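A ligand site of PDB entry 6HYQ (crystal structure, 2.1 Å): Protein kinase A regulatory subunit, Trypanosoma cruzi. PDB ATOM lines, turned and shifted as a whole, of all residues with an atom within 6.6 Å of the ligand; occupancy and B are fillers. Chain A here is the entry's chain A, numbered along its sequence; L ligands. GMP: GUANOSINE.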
ATOM      1  N   MET A  73     -20.604 -32.946 -33.821  1.00  0.00           N
ATOM      2  CA  MET A  73     -20.459 -31.606 -34.375  1.00  0.00           C
ATOM      3  C   MET A  73     -18.967 -31.331 -34.511  1.00  0.00           C
ATOM      4  O   MET A  73     -18.114 -32.082 -34.004  1.00  0.00           O
ATOM      5  CB  MET A  73     -21.229 -30.567 -33.519  1.00  0.00           C
ATOM      6  CG  MET A  73     -20.924 -30.559 -32.004  1.00  0.00           C
ATOM      7  SD  MET A  73     -22.063 -29.559 -30.914  1.00  0.00           S
ATOM      8  CE  MET A  73     -23.538 -30.580 -30.735  1.00  0.00           C
ATOM      9  N   LEU A  83     -29.566 -29.619 -29.786  1.00  0.00           N
ATOM     10  CA  LEU A  83     -29.085 -29.903 -28.436  1.00  0.00           C
ATOM     11  C   LEU A  83     -29.146 -31.400 -28.184  1.00  0.00           C
ATOM     12  O   LEU A  83     -30.259 -31.967 -28.267  1.00  0.00           O
ATOM     13  CB  LEU A  83     -29.981 -29.219 -27.411  1.00  0.00           C
ATOM     14  CG  LEU A  83     -29.737 -29.523 -25.944  1.00  0.00           C
ATOM     15  CD1 LEU A  83     -28.399 -28.994 -25.526  1.00  0.00           C
ATOM     16  CD2 LEU A  83     -30.912 -28.909 -25.195  1.00  0.00           C
ATOM     17  N   ILE A  93     -14.316 -32.995 -25.860  1.00  0.00           N
ATOM     18  CA  ILE A  93     -14.393 -31.653 -26.411  1.00  0.00           C
ATOM     19  C   ILE A  93     -13.016 -31.260 -26.927  1.00  0.00           C
ATOM     20  O   ILE A  93     -12.031 -31.236 -26.185  1.00  0.00           O
ATOM     21  CB  ILE A  93     -14.885 -30.636 -25.354  1.00  0.00           C
ATOM     22  CG1 ILE A  93     -16.256 -31.033 -24.749  1.00  0.00           C
ATOM     23  CG2 ILE A  93     -14.921 -29.192 -25.958  1.00  0.00           C
ATOM     24  CD1 ILE A  93     -17.375 -31.094 -25.680  1.00  0.00           C
ATOM     25  N   LYS A  95     -10.899 -28.316 -28.866  1.00  0.00           N
ATOM     26  CA  LYS A  95     -10.784 -26.933 -29.315  1.00  0.00           C
ATOM     27  C   LYS A  95      -9.359 -26.663 -29.832  1.00  0.00           C
ATOM     28  O   LYS A  95      -8.425 -26.484 -29.045  1.00  0.00           O
ATOM     29  CB  LYS A  95     -11.145 -26.001 -28.166  1.00  0.00           C
ATOM     30  CG  LYS A  95     -12.628 -25.961 -27.877  1.00  0.00           C
ATOM     31  CD  LYS A  95     -13.118 -24.576 -27.528  1.00  0.00           C
ATOM     32  CE  LYS A  95     -12.800 -24.260 -26.094  1.00  0.00           C
ATOM     33  NZ  LYS A  95     -13.152 -22.879 -25.787  1.00  0.00           N
ATOM     34  N   VAL A 100     -10.084 -31.004 -24.509  1.00  0.00           N
ATOM     35  CA  VAL A 100     -10.168 -30.107 -23.356  1.00  0.00           C
ATOM     36  C   VAL A 100     -11.222 -30.544 -22.331  1.00  0.00           C
ATOM     37  O   VAL A 100     -11.156 -30.110 -21.167  1.00  0.00           O
ATOM     38  CB  VAL A 100     -10.423 -28.652 -23.794  1.00  0.00           C
ATOM     39  CG1 VAL A 100      -9.296 -28.183 -24.720  1.00  0.00           C
ATOM     40  CG2 VAL A 100     -11.792 -28.510 -24.422  1.00  0.00           C
ATOM     41  N   TYR A 101     -12.189 -31.401 -22.682  1.00  0.00           N
ATOM     42  CA  TYR A 101     -13.239 -31.795 -21.754  1.00  0.00           C
ATOM     43  C   TYR A 101     -13.850 -33.130 -22.153  1.00  0.00           C
ATOM     44  O   TYR A 101     -14.077 -33.416 -23.336  1.00  0.00           O
ATOM     45  CB  TYR A 101     -14.351 -30.719 -21.701  1.00  0.00           C
ATOM     46  CG  TYR A 101     -15.356 -30.877 -20.533  1.00  0.00           C
ATOM     47  CD1 TYR A 101     -15.112 -30.337 -19.276  1.00  0.00           C
ATOM     48  CD2 TYR A 101     -16.557 -31.522 -20.725  1.00  0.00           C
ATOM     49  CE1 TYR A 101     -16.037 -30.467 -18.279  1.00  0.00           C
ATOM     50  CE2 TYR A 101     -17.488 -31.626 -19.747  1.00  0.00           C
ATOM     51  CZ  TYR A 101     -17.226 -31.114 -18.519  1.00  0.00           C
ATOM     52  OH  TYR A 101     -18.175 -31.279 -17.534  1.00  0.00           O
ATOM     53  N   LEU A 102     -14.124 -33.952 -21.169  1.00  0.00           N
ATOM     54  CA  LEU A 102     -14.820 -35.216 -21.356  1.00  0.00           C
ATOM     55  C   LEU A 102     -16.290 -35.076 -20.942  1.00  0.00           C
ATOM     56  O   LEU A 102     -16.598 -34.699 -19.804  1.00  0.00           O
ATOM     57  CB  LEU A 102     -14.143 -36.316 -20.565  1.00  0.00           C
ATOM     58  CG  LEU A 102     -14.708 -37.697 -20.826  1.00  0.00           C
ATOM     59  CD1 LEU A 102     -14.502 -38.123 -22.238  1.00  0.00           C
ATOM     60  CD2 LEU A 102     -13.956 -38.612 -19.942  1.00  0.00           C
ATOM     61  N   LYS A 103     -17.182 -35.319 -21.896  1.00  0.00           N
ATOM     62  CA  LYS A 103     -18.623 -35.288 -21.707  1.00  0.00           C
ATOM     63  C   LYS A 103     -19.156 -36.708 -21.480  1.00  0.00           C
ATOM     64  O   LYS A 103     -19.168 -37.513 -22.403  1.00  0.00           O
ATOM     65  CB  LYS A 103     -19.310 -34.682 -22.916  1.00  0.00           C
ATOM     66  CG  LYS A 103     -19.006 -33.203 -23.047  1.00  0.00           C
ATOM     67  CD  LYS A 103     -20.052 -32.390 -22.272  1.00  0.00           C
ATOM     68  CE  LYS A 103     -19.733 -30.892 -22.405  1.00  0.00           C
ATOM     69  NZ  LYS A 103     -20.545 -29.999 -21.590  1.00  0.00           N
ATOM     70  N   ALA A 108     -24.675 -32.648 -21.917  1.00  0.00           N
ATOM     71  CA  ALA A 108     -25.251 -32.100 -23.128  1.00  0.00           C
ATOM     72  C   ALA A 108     -24.166 -31.416 -23.946  1.00  0.00           C
ATOM     73  O   ALA A 108     -23.239 -30.820 -23.401  1.00  0.00           O
ATOM     74  CB  ALA A 108     -26.374 -31.080 -22.836  1.00  0.00           C
ATOM     75  N   VAL A 109     -24.281 -31.526 -25.257  1.00  0.00           N
ATOM     76  CA  VAL A 109     -23.421 -30.756 -26.161  1.00  0.00           C
ATOM     77  C   VAL A 109     -24.369 -29.981 -27.073  1.00  0.00           C
ATOM     78  O   VAL A 109     -25.513 -30.417 -27.298  1.00  0.00           O
ATOM     79  CB  VAL A 109     -22.425 -31.661 -26.940  1.00  0.00           C
ATOM     80  CG1 VAL A 109     -21.426 -32.302 -26.030  1.00  0.00           C
ATOM     81  CG2 VAL A 109     -23.140 -32.751 -27.705  1.00  0.00           C
ATOM     82  N   GLY A 110     -23.971 -28.762 -27.457  1.00  0.00           N
ATOM     83  CA  GLY A 110     -24.790 -27.939 -28.329  1.00  0.00           C
ATOM     84  C   GLY A 110     -25.477 -26.794 -27.642  1.00  0.00           C
ATOM     85  O   GLY A 110     -26.100 -25.944 -28.317  1.00  0.00           O
ATOM     86  N   GLU A 111     -25.453 -26.740 -26.325  1.00  0.00           N
ATOM     87  CA  GLU A 111     -26.272 -25.721 -25.681  1.00  0.00           C
ATOM     88  C   GLU A 111     -25.660 -24.330 -25.888  1.00  0.00           C
ATOM     89  O   GLU A 111     -26.345 -23.314 -25.745  1.00  0.00           O
ATOM     90  CB  GLU A 111     -26.428 -26.057 -24.198  1.00  0.00           C
ATOM     91  CG  GLU A 111     -25.261 -25.573 -23.348  1.00  0.00           C
ATOM     92  CD  GLU A 111     -24.002 -26.399 -23.569  1.00  0.00           C
ATOM     93  OE1 GLU A 111     -22.979 -26.149 -22.929  1.00  0.00           O
ATOM     94  OE2 GLU A 111     -24.069 -27.393 -24.321  1.00  0.00           O
ATOM     95  N   LEU A 112     -24.338 -24.307 -26.016  1.00  0.00           N
ATOM     96  CA  LEU A 112     -23.590 -23.045 -26.148  1.00  0.00           C
ATOM     97  C   LEU A 112     -23.936 -22.327 -27.420  1.00  0.00           C
ATOM     98  O   LEU A 112     -24.176 -21.125 -27.403  1.00  0.00           O
ATOM     99  CB  LEU A 112     -22.088 -23.322 -26.091  1.00  0.00           C
ATOM    100  CG  LEU A 112     -21.059 -22.204 -25.874  1.00  0.00           C
ATOM    101  CD1 LEU A 112     -21.333 -21.518 -24.611  1.00  0.00           C
ATOM    102  CD2 LEU A 112     -19.691 -22.835 -25.793  1.00  0.00           C
ATOM    103  N   GLU A 113     -24.096 -23.081 -28.518  1.00  0.00           N
ATOM    104  CA  GLU A 113     -24.460 -22.521 -29.801  1.00  0.00           C
ATOM    105  C   GLU A 113     -25.889 -22.048 -29.789  1.00  0.00           C
ATOM    106  O   GLU A 113     -26.221 -21.023 -30.391  1.00  0.00           O
ATOM    107  CB  GLU A 113     -24.312 -23.609 -30.876  1.00  0.00           C
ATOM    108  CG  GLU A 113     -22.837 -24.022 -31.173  1.00  0.00           C
ATOM    109  CD  GLU A 113     -22.098 -24.801 -30.024  1.00  0.00           C
ATOM    110  OE1 GLU A 113     -22.733 -25.448 -29.139  1.00  0.00           O
ATOM    111  OE2 GLU A 113     -20.848 -24.736 -30.045  1.00  0.00           O
ATOM    112  N   LEU A 114     -26.760 -22.822 -29.093  1.00  0.00           N
ATOM    113  CA  LEU A 114     -28.157 -22.433 -28.958  1.00  0.00           C
ATOM    114  C   LEU A 114     -28.400 -21.226 -28.057  1.00  0.00           C
ATOM    115  O   LEU A 114     -29.403 -20.538 -28.210  1.00  0.00           O
ATOM    116  CB  LEU A 114     -28.982 -23.610 -28.432  1.00  0.00           C
ATOM    117  CG  LEU A 114     -28.951 -24.850 -29.331  1.00  0.00           C
ATOM    118  CD1 LEU A 114     -29.869 -25.876 -28.812  1.00  0.00           C
ATOM    119  CD2 LEU A 114     -29.294 -24.511 -30.814  1.00  0.00           C
ATOM    120  N   PRO A 119     -21.628 -20.252 -34.382  1.00  0.00           N
ATOM    121  CA  PRO A 119     -21.199 -21.562 -34.888  1.00  0.00           C
ATOM    122  C   PRO A 119     -20.587 -22.463 -33.818  1.00  0.00           C
ATOM    123  O   PRO A 119     -20.055 -21.999 -32.815  1.00  0.00           O
ATOM    124  CB  PRO A 119     -20.154 -21.205 -35.946  1.00  0.00           C
ATOM    125  CG  PRO A 119     -20.559 -19.863 -36.380  1.00  0.00           C
ATOM    126  CD  PRO A 119     -21.138 -19.164 -35.227  1.00  0.00           C
ATOM    127  N   VAL A 120     -20.704 -23.769 -34.028  1.00  0.00           N
ATOM    128  CA  VAL A 120     -20.073 -24.713 -33.116  1.00  0.00           C
ATOM    129  C   VAL A 120     -18.675 -24.166 -32.802  1.00  0.00           C
ATOM    130  O   VAL A 120     -17.947 -23.768 -33.697  1.00  0.00           O
ATOM    131  CB  VAL A 120     -20.026 -26.132 -33.714  1.00  0.00           C
ATOM    132  CG1 VAL A 120     -19.406 -27.150 -32.748  1.00  0.00           C
ATOM    133  CG2 VAL A 120     -21.416 -26.593 -34.177  1.00  0.00           C
ATOM    134  N   VAL A 121     -18.367 -24.078 -31.500  1.00  0.00           N
ATOM    135  CA  VAL A 121     -17.079 -23.611 -30.974  1.00  0.00           C
ATOM    136  C   VAL A 121     -16.086 -24.750 -30.830  1.00  0.00           C
ATOM    137  O   VAL A 121     -14.858 -24.533 -30.870  1.00  0.00           O
ATOM    138  CB  VAL A 121     -17.339 -22.947 -29.606  1.00  0.00           C
ATOM    139  CG1 VAL A 121     -16.049 -22.470 -28.983  1.00  0.00           C
ATOM    140  CG2 VAL A 121     -18.381 -21.802 -29.737  1.00  0.00           C
ATOM    141  N   ALA A 122     -16.555 -25.961 -30.605  1.00  0.00           N
ATOM    142  CA  ALA A 122     -15.631 -27.027 -30.333  1.00  0.00           C
ATOM    143  C   ALA A 122     -16.154 -28.307 -30.962  1.00  0.00           C
ATOM    144  O   ALA A 122     -17.350 -28.460 -31.181  1.00  0.00           O
ATOM    145  CB  ALA A 122     -15.466 -27.168 -28.816  1.00  0.00           C
ATOM    146  N   THR A 123     -15.245 -29.191 -31.250  1.00  0.00           N
ATOM    147  CA  THR A 123     -15.578 -30.470 -31.839  1.00  0.00           C
ATOM    148  C   THR A 123     -15.888 -31.509 -30.757  1.00  0.00           C
ATOM    149  O   THR A 123     -15.238 -31.564 -29.709  1.00  0.00           O
ATOM    150  CB  THR A 123     -14.410 -30.924 -32.705  1.00  0.00           C
ATOM    151  OG1 THR A 123     -14.263 -30.026 -33.802  1.00  0.00           O
ATOM    152  CG2 THR A 123     -14.605 -32.375 -33.191  1.00  0.00           C
ATOM    153  N   VAL A 124     -16.872 -32.362 -31.037  1.00  0.00           N
ATOM    154  CA  VAL A 124     -17.348 -33.356 -30.055  1.00  0.00           C
ATOM    155  C   VAL A 124     -17.115 -34.705 -30.684  1.00  0.00           C
ATOM    156  O   VAL A 124     -17.731 -35.054 -31.695  1.00  0.00           O
ATOM    157  CB  VAL A 124     -18.846 -33.146 -29.671  1.00  0.00           C
ATOM    158  CG1 VAL A 124     -19.317 -34.175 -28.666  1.00  0.00           C
ATOM    159  CG2 VAL A 124     -19.091 -31.731 -29.098  1.00  0.00           C
ATOM    160  N   ASP A 170     -13.897 -24.320 -13.663  1.00  0.00           N
ATOM    161  CA  ASP A 170     -13.508 -23.368 -14.702  1.00  0.00           C
ATOM    162  C   ASP A 170     -14.723 -22.513 -15.100  1.00  0.00           C
ATOM    163  O   ASP A 170     -15.816 -22.685 -14.560  1.00  0.00           O
ATOM    164  CB  ASP A 170     -12.814 -24.132 -15.822  1.00  0.00           C
ATOM    165  CG  ASP A 170     -13.704 -25.242 -16.467  1.00  0.00           C
ATOM    166  OD1 ASP A 170     -14.961 -25.074 -16.626  1.00  0.00           O
ATOM    167  OD2 ASP A 170     -13.103 -26.300 -16.813  1.00  0.00           O
ATOM    168  N   TYR A 172     -16.565 -22.510 -17.508  1.00  0.00           N
ATOM    169  CA  TYR A 172     -17.655 -23.256 -18.111  1.00  0.00           C
ATOM    170  C   TYR A 172     -18.441 -23.970 -17.028  1.00  0.00           C
ATOM    171  O   TYR A 172     -19.646 -23.894 -16.999  1.00  0.00           O
ATOM    172  CB  TYR A 172     -17.136 -24.215 -19.176  1.00  0.00           C
ATOM    173  CG  TYR A 172     -18.210 -25.072 -19.795  1.00  0.00           C
ATOM    174  CD1 TYR A 172     -18.688 -26.228 -19.164  1.00  0.00           C
ATOM    175  CD2 TYR A 172     -18.747 -24.732 -21.026  1.00  0.00           C
ATOM    176  CE1 TYR A 172     -19.670 -27.039 -19.764  1.00  0.00           C
ATOM    177  CE2 TYR A 172     -19.689 -25.546 -21.637  1.00  0.00           C
ATOM    178  CZ  TYR A 172     -20.162 -26.689 -21.001  1.00  0.00           C
ATOM    179  OH  TYR A 172     -21.167 -27.418 -21.626  1.00  0.00           O
ATOM    180  N   GLU A 173     -17.753 -24.489 -16.044  1.00  0.00           N
ATOM    181  CA  GLU A 173     -18.428 -25.219 -14.969  1.00  0.00           C
ATOM    182  C   GLU A 173     -19.197 -24.253 -14.051  1.00  0.00           C
ATOM    183  O   GLU A 173     -20.303 -24.578 -13.558  1.00  0.00           O
ATOM    184  CB  GLU A 173     -17.372 -26.045 -14.239  1.00  0.00           C
ATOM    185  CG  GLU A 173     -16.800 -27.185 -15.137  1.00  0.00           C
ATOM    186  CD  GLU A 173     -15.540 -27.778 -14.587  1.00  0.00           C
ATOM    187  OE1 GLU A 173     -14.745 -27.046 -13.953  1.00  0.00           O
ATOM    188  OE2 GLU A 173     -15.351 -28.988 -14.742  1.00  0.00           O
HETATM  189  O5' GMP L   1     -18.998 -26.385 -28.940  1.00  0.00           O
HETATM  190  C5' GMP L   1     -19.824 -27.543 -28.982  1.00  0.00           C
HETATM  191  C4' GMP L   1     -20.207 -28.035 -27.600  1.00  0.00           C
HETATM  192  O4' GMP L   1     -19.016 -28.388 -26.853  1.00  0.00           O
HETATM  193  C3' GMP L   1     -20.960 -27.050 -26.683  1.00  0.00           C
HETATM  194  O3' GMP L   1     -22.350 -27.012 -26.939  1.00  0.00           O
HETATM  195  C2' GMP L   1     -20.628 -27.548 -25.280  1.00  0.00           C
HETATM  196  O2' GMP L   1     -21.537 -28.593 -24.846  1.00  0.00           O
HETATM  197  C1' GMP L   1     -19.204 -28.093 -25.474  1.00  0.00           C
HETATM  198  N9  GMP L   1     -18.208 -27.080 -25.160  1.00  0.00           N
HETATM  199  C8  GMP L   1     -17.834 -26.092 -26.007  1.00  0.00           C
HETATM  200  N7  GMP L   1     -16.879 -25.366 -25.409  1.00  0.00           N
HETATM  201  C5  GMP L   1     -16.707 -25.939 -24.217  1.00  0.00           C
HETATM  202  C6  GMP L   1     -15.777 -25.625 -23.068  1.00  0.00           C
HETATM  203  O6  GMP L   1     -15.026 -24.679 -23.132  1.00  0.00           O
HETATM  204  N1  GMP L   1     -15.813 -26.474 -21.913  1.00  0.00           N
HETATM  205  C2  GMP L   1     -16.704 -27.581 -21.775  1.00  0.00           C
HETATM  206  N2  GMP L   1     -16.642 -28.314 -20.518  1.00  0.00           N
HETATM  207  N3  GMP L   1     -17.559 -27.901 -22.856  1.00  0.00           N
HETATM  208  C4  GMP L   1     -17.532 -27.015 -24.056  1.00  0.00           C
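The backbone NH of Tyr 172 lies close to the side-chain carboxylate of Asp 170 (3.2 Å).
O of Ile 93 lies within hydrogen-bond range of N of Val 100, at 2.6 Å.
The backbone NH (N) of Val 124 lies within hydrogen-bond range of the backbone carbonyl oxygen (O) of Met 73, 3.2 Å away.
The backbone carbonyl oxygen (O) of Tyr 101 is in hydrogen-bond range of the backbone NH (N) of Ile 93.
N of Val 121 is in hydrogen-bond range of OE2 of Glu 113, 3.0 Å away.
The side-chain hydroxyl of Tyr 172 lies within hydrogen-bond range of the side-chain carboxylate of Glu 111 (2.6 Å).
The side-chain hydroxyl (OH) of Tyr 172 is in hydrogen-bond range of the side-chain amino group (NZ) of Lys 103 (2.7 Å).
O of Ala 108 is in hydrogen-bond range of NZ of Lys 103 (3.3 Å).
Residues that only touch the ligand: Tyr 101 (2.8 Å), Val 109 (3.2 Å), Ile 93 (3.4 Å), Val 121 (3.5 Å), Met 73 (3.6 Å), Lys 103 (3.7 Å), Lys 95 (3.7 Å) and Val 120 (3.8 Å).
Hydrophobic or aromatic side chains that line the ligand: Met 73, Ile 93, Tyr 101, Val 109, Leu 112, Val 120, Val 121, Ala 122 and Tyr 172.
15 residues have an atom within 4 Å of the ligand: Met 73, Ile 93, Lys 95, Tyr 101, Lys 103, Ala 108, Val 109, Gly 110, Glu 111, Leu 112, Glu 113, Val 120, Val 121, Ala 122 and Tyr 172.
O3' of the ligand sits at hydrogen-bond distance from N of Leu 112 (3.5 Å).
The backbone NH of Gly 110 is in hydrogen-bond range of an oxygen (O3') of the ligand (2.4 Å).
O2' of the ligand sits at hydrogen-bond distance from OE2 of Glu 111 (2.9 Å).
An oxygen (O2') of the ligand lies within hydrogen-bond range of the backbone carbonyl oxygen (O) of Ala 108 (3.2 Å).
O3' of the ligand sits at hydrogen-bond distance from N of Glu 111 (3.2 Å).
An oxygen (O2') of the ligand is in hydrogen-bond range of the side-chain hydroxyl of Tyr 172 (3.4 Å).
The side-chain carboxylate (OE2) of Glu 113 lies within hydrogen-bond range of an oxygen (O5') of the ligand (2.7 Å).
O5' of the ligand lies close to O of Ala 122.
N of Ala 122 sits at hydrogen-bond distance from O5' of the ligand, 3.0 Å away.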
